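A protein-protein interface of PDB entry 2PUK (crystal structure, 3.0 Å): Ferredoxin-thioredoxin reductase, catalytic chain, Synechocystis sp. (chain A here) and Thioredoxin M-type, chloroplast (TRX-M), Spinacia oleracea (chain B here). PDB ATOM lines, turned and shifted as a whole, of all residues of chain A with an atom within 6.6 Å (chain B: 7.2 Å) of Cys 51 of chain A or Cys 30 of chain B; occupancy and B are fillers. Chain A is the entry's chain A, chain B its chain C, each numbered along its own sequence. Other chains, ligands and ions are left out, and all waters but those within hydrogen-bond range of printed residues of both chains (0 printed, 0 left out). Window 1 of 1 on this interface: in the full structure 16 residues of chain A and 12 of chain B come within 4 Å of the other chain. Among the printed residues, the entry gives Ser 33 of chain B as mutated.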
ATOM      1  N   VAL A  29      11.953  22.267 -12.037  1.00  0.00           N
ATOM      2  CA  VAL A  29      13.188  21.513 -12.263  1.00  0.00           C
ATOM      3  C   VAL A  29      14.035  22.174 -13.343  1.00  0.00           C
ATOM      4  O   VAL A  29      15.240  22.369 -13.160  1.00  0.00           O
ATOM      5  CB  VAL A  29      12.889  20.035 -12.614  1.00  0.00           C
ATOM      6  CG1 VAL A  29      13.916  19.456 -13.590  1.00  0.00           C
ATOM      7  CG2 VAL A  29      12.817  19.208 -11.345  1.00  0.00           C
ATOM      8  N   VAL A  32      15.448  25.356 -11.846  1.00  0.00           N
ATOM      9  CA  VAL A  32      16.593  25.123 -10.973  1.00  0.00           C
ATOM     10  C   VAL A  32      17.891  25.017 -11.783  1.00  0.00           C
ATOM     11  O   VAL A  32      18.847  25.745 -11.519  1.00  0.00           O
ATOM     12  CB  VAL A  32      16.360  23.895 -10.052  1.00  0.00           C
ATOM     13  CG1 VAL A  32      17.661  23.372  -9.465  1.00  0.00           C
ATOM     14  CG2 VAL A  32      15.420  24.271  -8.935  1.00  0.00           C
ATOM     15  N   VAL A  33      17.897  24.141 -12.787  1.00  0.00           N
ATOM     16  CA  VAL A  33      19.076  23.914 -13.627  1.00  0.00           C
ATOM     17  C   VAL A  33      19.564  25.209 -14.280  1.00  0.00           C
ATOM     18  O   VAL A  33      20.715  25.609 -14.095  1.00  0.00           O
ATOM     19  CB  VAL A  33      18.811  22.849 -14.719  1.00  0.00           C
ATOM     20  CG1 VAL A  33      20.055  22.629 -15.564  1.00  0.00           C
ATOM     21  CG2 VAL A  33      18.357  21.544 -14.096  1.00  0.00           C
ATOM     22  N   GLY A  36      21.250  27.391 -11.962  1.00  0.00           N
ATOM     23  CA  GLY A  36      22.529  26.805 -11.556  1.00  0.00           C
ATOM     24  C   GLY A  36      23.595  26.984 -12.619  1.00  0.00           C
ATOM     25  O   GLY A  36      24.764  27.208 -12.305  1.00  0.00           O
ATOM     26  N   HIS A  40      26.955  29.439 -12.289  1.00  0.00           N
ATOM     27  CA  HIS A  40      28.250  28.900 -12.681  1.00  0.00           C
ATOM     28  C   HIS A  40      28.869  29.746 -13.787  1.00  0.00           C
ATOM     29  O   HIS A  40      30.087  29.930 -13.837  1.00  0.00           O
ATOM     30  CB  HIS A  40      28.115  27.433 -13.103  1.00  0.00           C
ATOM     31  CG  HIS A  40      28.158  26.469 -11.956  1.00  0.00           C
ATOM     32  ND1 HIS A  40      28.870  25.292 -12.002  1.00  0.00           N
ATOM     33  CD2 HIS A  40      27.595  26.518 -10.726  1.00  0.00           C
ATOM     34  CE1 HIS A  40      28.738  24.653 -10.855  1.00  0.00           C
ATOM     35  NE2 HIS A  40      27.970  25.377 -10.062  1.00  0.00           N
ATOM     36  N   LEU A  48      29.096  25.833 -16.302  1.00  0.00           N
ATOM     37  CA  LEU A  48      29.485  24.495 -15.873  1.00  0.00           C
ATOM     38  C   LEU A  48      28.291  23.758 -15.280  1.00  0.00           C
ATOM     39  O   LEU A  48      27.575  24.312 -14.448  1.00  0.00           O
ATOM     40  CB  LEU A  48      30.602  24.591 -14.836  1.00  0.00           C
ATOM     41  CG  LEU A  48      31.790  23.629 -14.842  1.00  0.00           C
ATOM     42  CD1 LEU A  48      32.334  23.528 -13.435  1.00  0.00           C
ATOM     43  CD2 LEU A  48      31.451  22.245 -15.358  1.00  0.00           C
ATOM     44  N   CYS A  49      28.092  22.510 -15.707  1.00  0.00           N
ATOM     45  CA  CYS A  49      26.939  21.698 -15.302  1.00  0.00           C
ATOM     46  C   CYS A  49      26.690  21.693 -13.793  1.00  0.00           C
ATOM     47  O   CYS A  49      27.593  21.382 -13.016  1.00  0.00           O
ATOM     48  CB  CYS A  49      27.087  20.263 -15.805  1.00  0.00           C
ATOM     49  SG  CYS A  49      25.559  19.308 -15.702  1.00  0.00           S
ATOM     50  N   PRO A  50      25.457  22.033 -13.377  1.00  0.00           N
ATOM     51  CA  PRO A  50      25.148  22.185 -11.964  1.00  0.00           C
ATOM     52  C   PRO A  50      24.724  20.883 -11.312  1.00  0.00           C
ATOM     53  O   PRO A  50      24.365  20.881 -10.137  1.00  0.00           O
ATOM     54  CB  PRO A  50      23.973  23.159 -11.980  1.00  0.00           C
ATOM     55  CG  PRO A  50      23.249  22.826 -13.242  1.00  0.00           C
ATOM     56  CD  PRO A  50      24.277  22.302 -14.222  1.00  0.00           C
ATOM     57  N   CYS A  51      24.751  19.790 -12.069  1.00  0.00           N
ATOM     58  CA  CYS A  51      24.400  18.482 -11.528  1.00  0.00           C
ATOM     59  C   CYS A  51      25.576  17.515 -11.477  1.00  0.00           C
ATOM     60  O   CYS A  51      25.432  16.331 -11.767  1.00  0.00           O
ATOM     61  CB  CYS A  51      23.216  17.878 -12.275  1.00  0.00           C
ATOM     62  SG  CYS A  51      21.646  18.610 -11.774  1.00  0.00           S
ATOM     63  N   ARG A  52      26.736  18.034 -11.095  1.00  0.00           N
ATOM     64  CA  ARG A  52      27.882  17.199 -10.777  1.00  0.00           C
ATOM     65  C   ARG A  52      28.681  17.811  -9.637  1.00  0.00           C
ATOM     66  O   ARG A  52      28.531  18.991  -9.325  1.00  0.00           O
ATOM     67  CB  ARG A  52      28.787  16.986 -11.992  1.00  0.00           C
ATOM     68  CG  ARG A  52      28.091  16.405 -13.200  1.00  0.00           C
ATOM     69  CD  ARG A  52      29.035  15.620 -14.071  1.00  0.00           C
ATOM     70  NE  ARG A  52      28.803  14.182 -13.984  1.00  0.00           N
ATOM     71  CZ  ARG A  52      29.729  13.286 -13.662  1.00  0.00           C
ATOM     72  NH1 ARG A  52      30.974  13.669 -13.399  1.00  0.00           N
ATOM     73  NH2 ARG A  52      29.409  12.002 -13.614  1.00  0.00           N
ATOM     74  N   HIS A  53      29.510  16.987  -9.005  1.00  0.00           N
ATOM     75  CA  HIS A  53      30.492  17.454  -8.043  1.00  0.00           C
ATOM     76  C   HIS A  53      31.845  17.506  -8.743  1.00  0.00           C
ATOM     77  O   HIS A  53      32.177  16.626  -9.541  1.00  0.00           O
ATOM     78  CB  HIS A  53      30.539  16.533  -6.815  1.00  0.00           C
ATOM     79  CG  HIS A  53      31.751  16.727  -5.958  1.00  0.00           C
ATOM     80  ND1 HIS A  53      31.863  17.757  -5.048  1.00  0.00           N
ATOM     81  CD2 HIS A  53      32.913  16.033  -5.884  1.00  0.00           C
ATOM     82  CE1 HIS A  53      33.039  17.689  -4.448  1.00  0.00           C
ATOM     83  NE2 HIS A  53      33.696  16.652  -4.937  1.00  0.00           N
ATOM     84  N   TYR A  54      32.618  18.547  -8.446  1.00  0.00           N
ATOM     85  CA  TYR A  54      33.930  18.729  -9.056  1.00  0.00           C
ATOM     86  C   TYR A  54      35.025  18.892  -8.007  1.00  0.00           C
ATOM     87  O   TYR A  54      34.866  19.640  -7.036  1.00  0.00           O
ATOM     88  CB  TYR A  54      33.922  19.940  -9.997  1.00  0.00           C
ATOM     89  CG  TYR A  54      32.800  19.929 -11.010  1.00  0.00           C
ATOM     90  CD1 TYR A  54      31.645  20.679 -10.798  1.00  0.00           C
ATOM     91  CD2 TYR A  54      32.890  19.165 -12.173  1.00  0.00           C
ATOM     92  CE1 TYR A  54      30.609  20.679 -11.719  1.00  0.00           C
ATOM     93  CE2 TYR A  54      31.859  19.157 -13.103  1.00  0.00           C
ATOM     94  CZ  TYR A  54      30.722  19.915 -12.866  1.00  0.00           C
ATOM     95  OH  TYR A  54      29.694  19.913 -13.775  1.00  0.00           O
ATOM     96  N   HIS A  80      21.670  14.705 -17.853  1.00  0.00           N
ATOM     97  CA  HIS A  80      21.263  14.179 -16.555  1.00  0.00           C
ATOM     98  C   HIS A  80      20.711  15.219 -15.568  1.00  0.00           C
ATOM     99  O   HIS A  80      20.152  14.846 -14.532  1.00  0.00           O
ATOM    100  CB  HIS A  80      22.362  13.310 -15.933  1.00  0.00           C
ATOM    101  CG  HIS A  80      23.653  14.029 -15.717  1.00  0.00           C
ATOM    102  ND1 HIS A  80      24.000  14.582 -14.504  1.00  0.00           N
ATOM    103  CD2 HIS A  80      24.685  14.282 -16.557  1.00  0.00           C
ATOM    104  CE1 HIS A  80      25.189  15.149 -14.607  1.00  0.00           C
ATOM    105  NE2 HIS A  80      25.628  14.980 -15.841  1.00  0.00           N
ATOM    106  N   CYS A  81      20.860  16.506 -15.882  1.00  0.00           N
ATOM    107  CA  CYS A  81      20.171  17.555 -15.125  1.00  0.00           C
ATOM    108  C   CYS A  81      18.691  17.554 -15.484  1.00  0.00           C
ATOM    109  O   CYS A  81      17.876  18.180 -14.802  1.00  0.00           O
ATOM    110  CB  CYS A  81      20.716  18.938 -15.452  1.00  0.00           C
ATOM    111  SG  CYS A  81      22.467  19.158 -15.252  1.00  0.00           S
ATOM    112  N   MET A  82      18.362  16.860 -16.572  1.00  0.00           N
ATOM    113  CA  MET A  82      17.014  16.847 -17.138  1.00  0.00           C
ATOM    114  C   MET A  82      16.584  18.252 -17.556  1.00  0.00           C
ATOM    115  O   MET A  82      15.473  18.704 -17.269  1.00  0.00           O
ATOM    116  CB  MET A  82      16.012  16.202 -16.176  1.00  0.00           C
ATOM    117  CG  MET A  82      16.209  14.709 -15.995  1.00  0.00           C
ATOM    118  SD  MET A  82      15.502  14.129 -14.451  1.00  0.00           S
ATOM    119  CE  MET A  82      13.771  14.498 -14.679  1.00  0.00           C
ATOM    120  N   TRP B  26      23.129  15.451  -2.565  1.00  0.00           N
ATOM    121  CA  TRP B  26      22.362  16.429  -3.336  1.00  0.00           C
ATOM    122  C   TRP B  26      23.086  17.776  -3.443  1.00  0.00           C
ATOM    123  O   TRP B  26      24.162  17.965  -2.858  1.00  0.00           O
ATOM    124  CB  TRP B  26      20.962  16.613  -2.723  1.00  0.00           C
ATOM    125  CG  TRP B  26      20.933  17.499  -1.496  1.00  0.00           C
ATOM    126  CD1 TRP B  26      21.595  17.291  -0.320  1.00  0.00           C
ATOM    127  CD2 TRP B  26      20.200  18.722  -1.331  1.00  0.00           C
ATOM    128  NE1 TRP B  26      21.333  18.310   0.563  1.00  0.00           N
ATOM    129  CE2 TRP B  26      20.477  19.201  -0.028  1.00  0.00           C
ATOM    130  CE3 TRP B  26      19.337  19.460  -2.155  1.00  0.00           C
ATOM    131  CZ2 TRP B  26      19.921  20.386   0.472  1.00  0.00           C
ATOM    132  CZ3 TRP B  26      18.783  20.649  -1.654  1.00  0.00           C
ATOM    133  CH2 TRP B  26      19.081  21.095  -0.352  1.00  0.00           C
ATOM    134  N   ALA B  27      22.481  18.696  -4.201  1.00  0.00           N
ATOM    135  CA  ALA B  27      22.986  20.065  -4.406  1.00  0.00           C
ATOM    136  C   ALA B  27      21.820  21.025  -4.678  1.00  0.00           C
ATOM    137  O   ALA B  27      20.928  20.710  -5.476  1.00  0.00           O
ATOM    138  CB  ALA B  27      23.998  20.109  -5.556  1.00  0.00           C
ATOM    139  N   PRO B  28      21.826  22.203  -4.019  1.00  0.00           N
ATOM    140  CA  PRO B  28      20.733  23.189  -4.084  1.00  0.00           C
ATOM    141  C   PRO B  28      20.329  23.629  -5.497  1.00  0.00           C
ATOM    142  O   PRO B  28      19.228  24.153  -5.685  1.00  0.00           O
ATOM    143  CB  PRO B  28      21.298  24.387  -3.311  1.00  0.00           C
ATOM    144  CG  PRO B  28      22.289  23.807  -2.386  1.00  0.00           C
ATOM    145  CD  PRO B  28      22.916  22.667  -3.140  1.00  0.00           C
ATOM    146  N   TRP B  29      21.209  23.430  -6.477  1.00  0.00           N
ATOM    147  CA  TRP B  29      20.924  23.853  -7.845  1.00  0.00           C
ATOM    148  C   TRP B  29      21.002  22.710  -8.853  1.00  0.00           C
ATOM    149  O   TRP B  29      21.336  22.917 -10.021  1.00  0.00           O
ATOM    150  CB  TRP B  29      21.814  25.037  -8.244  1.00  0.00           C
ATOM    151  CG  TRP B  29      21.644  26.218  -7.332  1.00  0.00           C
ATOM    152  CD1 TRP B  29      22.574  26.726  -6.470  1.00  0.00           C
ATOM    153  CD2 TRP B  29      20.463  27.017  -7.166  1.00  0.00           C
ATOM    154  NE1 TRP B  29      22.053  27.801  -5.786  1.00  0.00           N
ATOM    155  CE2 TRP B  29      20.760  28.003  -6.194  1.00  0.00           C
ATOM    156  CE3 TRP B  29      19.187  27.002  -7.749  1.00  0.00           C
ATOM    157  CZ2 TRP B  29      19.828  28.967  -5.789  1.00  0.00           C
ATOM    158  CZ3 TRP B  29      18.256  27.963  -7.345  1.00  0.00           C
ATOM    159  CH2 TRP B  29      18.586  28.931  -6.373  1.00  0.00           C
ATOM    160  N   CYS B  30      20.678  21.505  -8.392  1.00  0.00           N
ATOM    161  CA  CYS B  30      20.534  20.361  -9.282  1.00  0.00           C
ATOM    162  C   CYS B  30      19.070  19.967  -9.426  1.00  0.00           C
ATOM    163  O   CYS B  30      18.412  19.612  -8.446  1.00  0.00           O
ATOM    164  CB  CYS B  30      21.355  19.166  -8.806  1.00  0.00           C
ATOM    165  SG  CYS B  30      21.257  17.769  -9.948  1.00  0.00           S
ATOM    166  N   GLY B  31      18.576  20.040 -10.658  1.00  0.00           N
ATOM    167  CA  GLY B  31      17.182  19.742 -10.974  1.00  0.00           C
ATOM    168  C   GLY B  31      16.661  18.512 -10.258  1.00  0.00           C
ATOM    169  O   GLY B  31      15.900  18.641  -9.297  1.00  0.00           O
ATOM    170  N   PRO B  32      17.092  17.314 -10.703  1.00  0.00           N
ATOM    171  CA  PRO B  32      16.665  16.038 -10.142  1.00  0.00           C
ATOM    172  C   PRO B  32      16.739  15.956  -8.622  1.00  0.00           C
ATOM    173  O   PRO B  32      16.005  15.173  -8.032  1.00  0.00           O
ATOM    174  CB  PRO B  32      17.639  15.048 -10.768  1.00  0.00           C
ATOM    175  CG  PRO B  32      17.947  15.645 -12.074  1.00  0.00           C
ATOM    176  CD  PRO B  32      18.044  17.112 -11.808  1.00  0.00           C
ATOM    177  N   SER B  33      17.606  16.755  -7.997  1.00  0.00           N
ATOM    178  CA  SER B  33      17.680  16.829  -6.533  1.00  0.00           C
ATOM    179  C   SER B  33      16.326  17.191  -5.938  1.00  0.00           C
ATOM    180  O   SER B  33      15.919  16.621  -4.921  1.00  0.00           O
ATOM    181  CB  SER B  33      18.733  17.839  -6.073  1.00  0.00           C
ATOM    182  OG  SER B  33      20.043  17.392  -6.361  1.00  0.00           O
ATOM    183  N   LYS B  34      15.638  18.135  -6.581  1.00  0.00           N
ATOM    184  CA  LYS B  34      14.279  18.512  -6.202  1.00  0.00           C
ATOM    185  C   LYS B  34      13.291  17.356  -6.353  1.00  0.00           C
ATOM    186  O   LYS B  34      12.284  17.304  -5.643  1.00  0.00           O
ATOM    187  CB  LYS B  34      13.798  19.698  -7.036  1.00  0.00           C
ATOM    188  CG  LYS B  34      13.766  21.016  -6.293  1.00  0.00           C
ATOM    189  CD  LYS B  34      13.123  22.110  -7.142  1.00  0.00           C
ATOM    190  CE  LYS B  34      11.602  22.023  -7.157  1.00  0.00           C
ATOM    191  NZ  LYS B  34      10.999  22.547  -5.899  1.00  0.00           N
ATOM    192  N   LEU B  35      13.584  16.439  -7.276  1.00  0.00           N
ATOM    193  CA  LEU B  35      12.687  15.318  -7.576  1.00  0.00           C
ATOM    194  C   LEU B  35      12.772  14.122  -6.618  1.00  0.00           C
ATOM    195  O   LEU B  35      11.739  13.577  -6.232  1.00  0.00           O
ATOM    196  CB  LEU B  35      12.850  14.870  -9.031  1.00  0.00           C
ATOM    197  CG  LEU B  35      11.717  15.228  -9.997  1.00  0.00           C
ATOM    198  CD1 LEU B  35      10.900  16.444  -9.547  1.00  0.00           C
ATOM    199  CD2 LEU B  35      12.263  15.430 -11.398  1.00  0.00           C
ATOM    200  N   ARG B  71      30.489  11.879  -7.853  1.00  0.00           N
ATOM    201  CA  ARG B  71      30.708  12.653  -9.065  1.00  0.00           C
ATOM    202  C   ARG B  71      29.416  13.164  -9.695  1.00  0.00           C
ATOM    203  O   ARG B  71      29.223  14.369  -9.824  1.00  0.00           O
ATOM    204  CB  ARG B  71      31.548  11.865 -10.064  1.00  0.00           C
ATOM    205  CG  ARG B  71      33.046  12.042  -9.895  1.00  0.00           C
ATOM    206  CD  ARG B  71      33.726  11.561 -11.164  1.00  0.00           C
ATOM    207  NE  ARG B  71      35.172  11.760 -11.189  1.00  0.00           N
ATOM    208  CZ  ARG B  71      36.066  10.872 -10.763  1.00  0.00           C
ATOM    209  NH1 ARG B  71      35.679   9.710 -10.257  1.00  0.00           N
ATOM    210  NH2 ARG B  71      37.358  11.150 -10.836  1.00  0.00           N
ATOM    211  N   SER B  72      28.534  12.254 -10.089  1.00  0.00           N
ATOM    212  CA  SER B  72      27.227  12.643 -10.594  1.00  0.00           C
ATOM    213  C   SER B  72      26.308  12.897  -9.407  1.00  0.00           C
ATOM    214  O   SER B  72      26.493  12.301  -8.352  1.00  0.00           O
ATOM    215  CB  SER B  72      26.660  11.551 -11.494  1.00  0.00           C
ATOM    216  OG  SER B  72      25.412  11.942 -12.028  1.00  0.00           O
ATOM    217  N   ILE B  73      25.338  13.794  -9.567  1.00  0.00           N
ATOM    218  CA  ILE B  73      24.340  14.060  -8.518  1.00  0.00           C
ATOM    219  C   ILE B  73      22.913  14.240  -9.072  1.00  0.00           C
ATOM    220  O   ILE B  73      22.734  14.788 -10.164  1.00  0.00           O
ATOM    221  CB  ILE B  73      24.732  15.253  -7.584  1.00  0.00           C
ATOM    222  CG1 ILE B  73      25.333  16.408  -8.377  1.00  0.00           C
ATOM    223  CG2 ILE B  73      25.697  14.793  -6.502  1.00  0.00           C
ATOM    224  CD1 ILE B  73      25.909  17.530  -7.524  1.00  0.00           C
ATOM    225  N   PRO B  74      21.892  13.782  -8.316  1.00  0.00           N
ATOM    226  CA  PRO B  74      22.040  13.194  -6.989  1.00  0.00           C
ATOM    227  C   PRO B  74      22.538  11.761  -7.061  1.00  0.00           C
ATOM    228  O   PRO B  74      22.179  11.032  -7.989  1.00  0.00           O
ATOM    229  CB  PRO B  74      20.615  13.241  -6.407  1.00  0.00           C
ATOM    230  CG  PRO B  74      19.764  13.944  -7.435  1.00  0.00           C
ATOM    231  CD  PRO B  74      20.480  13.812  -8.733  1.00  0.00           C
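SG of Cys 51 of chain A forms a disulfide with SG of Cys 30 of chain B, 2.0 Å away.
SG of Cys 51 of chain A sits at hydrogen-bond distance from N of Gly 31 of chain B (3.6 Å).
The backbone carbonyl oxygen (O) of Cys 51 of chain A sits at hydrogen-bond distance from the backbone NH (N) of Ile 73 of chain B (3.4 Å).
O of Arg 71 of chain B sits at hydrogen-bond distance from N of His 53 of chain A (2.8 Å).
N of Cys 51 of chain A lies close to SG of Cys 49 of chain A (3.8 Å).
SG of Cys 49 of chain A lies close to SG of Cys 81 of chain A (3.1 Å).
The side-chain sulfur (SG) of Cys 51 of chain A lies close to the side-chain sulfur (SG) of Cys 81 of chain A (3.6 Å).
O of Cys 30 of chain B lies close to OG of Ser 33 of chain B (3.5 Å).
Cys 51 of chain A touches just these residues of chain B: Cys 30, Gly 31, Pro 32 and Ile 73.
Tyr 54 of chain A touches none of the printed residues of chain B.
Of the printed residues of chain B, His 80 of chain A touches Pro 32 (3.4 Å) and Ser 72 (3.9 Å).
Of the printed residues of chain B, Cys 81 of chain A touches Pro 32 (3.2 Å).
Printed residues of chain B within 4 Å of Met 82 of chain A: Pro 32 and Leu 35.
Cys 30 of chain B touches just these residues of chain A: Val 32, Pro 50 and Cys 51.
Printed residues of chain A within 4 Å of Lys 34 of chain B: Val 32 (3.6 Å).
The nearest residue of chain B that does not touch Cys 51 of chain A is Ser 72 of chain B (4.3 Å).
The nearest residue of chain A that does not touch Cys 30 of chain B is Val 33 of chain A (5.0 Å).
Printed residues of chain B that touch a printed residue of chain A: Trp 29, Cys 30, Gly 31, Pro 32, Lys 34, Leu 35, Arg 71, Ser 72 and Ile 73.
Hydrophobic or aromatic side chains of chain A within 4 Å of the printed part of chain B: Val 29, Val 32, Val 33, Pro 50, His 53, His 80 and Met 82.
Among the printed residues, no Asp or Glu carboxylate lies within 4 Å of a Lys or Arg side-chain nitrogen of the other chain.
Val 29 of chain A touches Gly 31 of chain B (CG2 to O, 3.7 Å).
C of Trp 29 of chain B touches CG1 of Val 32 of chain A, at 3.5 Å.
Cys 30 of chain B touches Val 32 of chain A.
Val 32 of chain A touches Gly 31 of chain B.
Lys 34 of chain B touches Val 32 of chain A (CD to CG2, 3.6 Å).
Gly 31 of chain B touches Val 33 of chain A (N to CG2, 3.8 Å).
Pro 50 of chain A touches Trp 29 of chain B (CB to O, 3.3 Å).
Cys 30 of chain B touches Pro 50 of chain A (CB to O, 3.7 Å).
His 80 of chain A touches Pro 32 of chain B.
CG of Pro 32 of chain B touches SD of Met 82 of chain A, at 3.7 Å.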
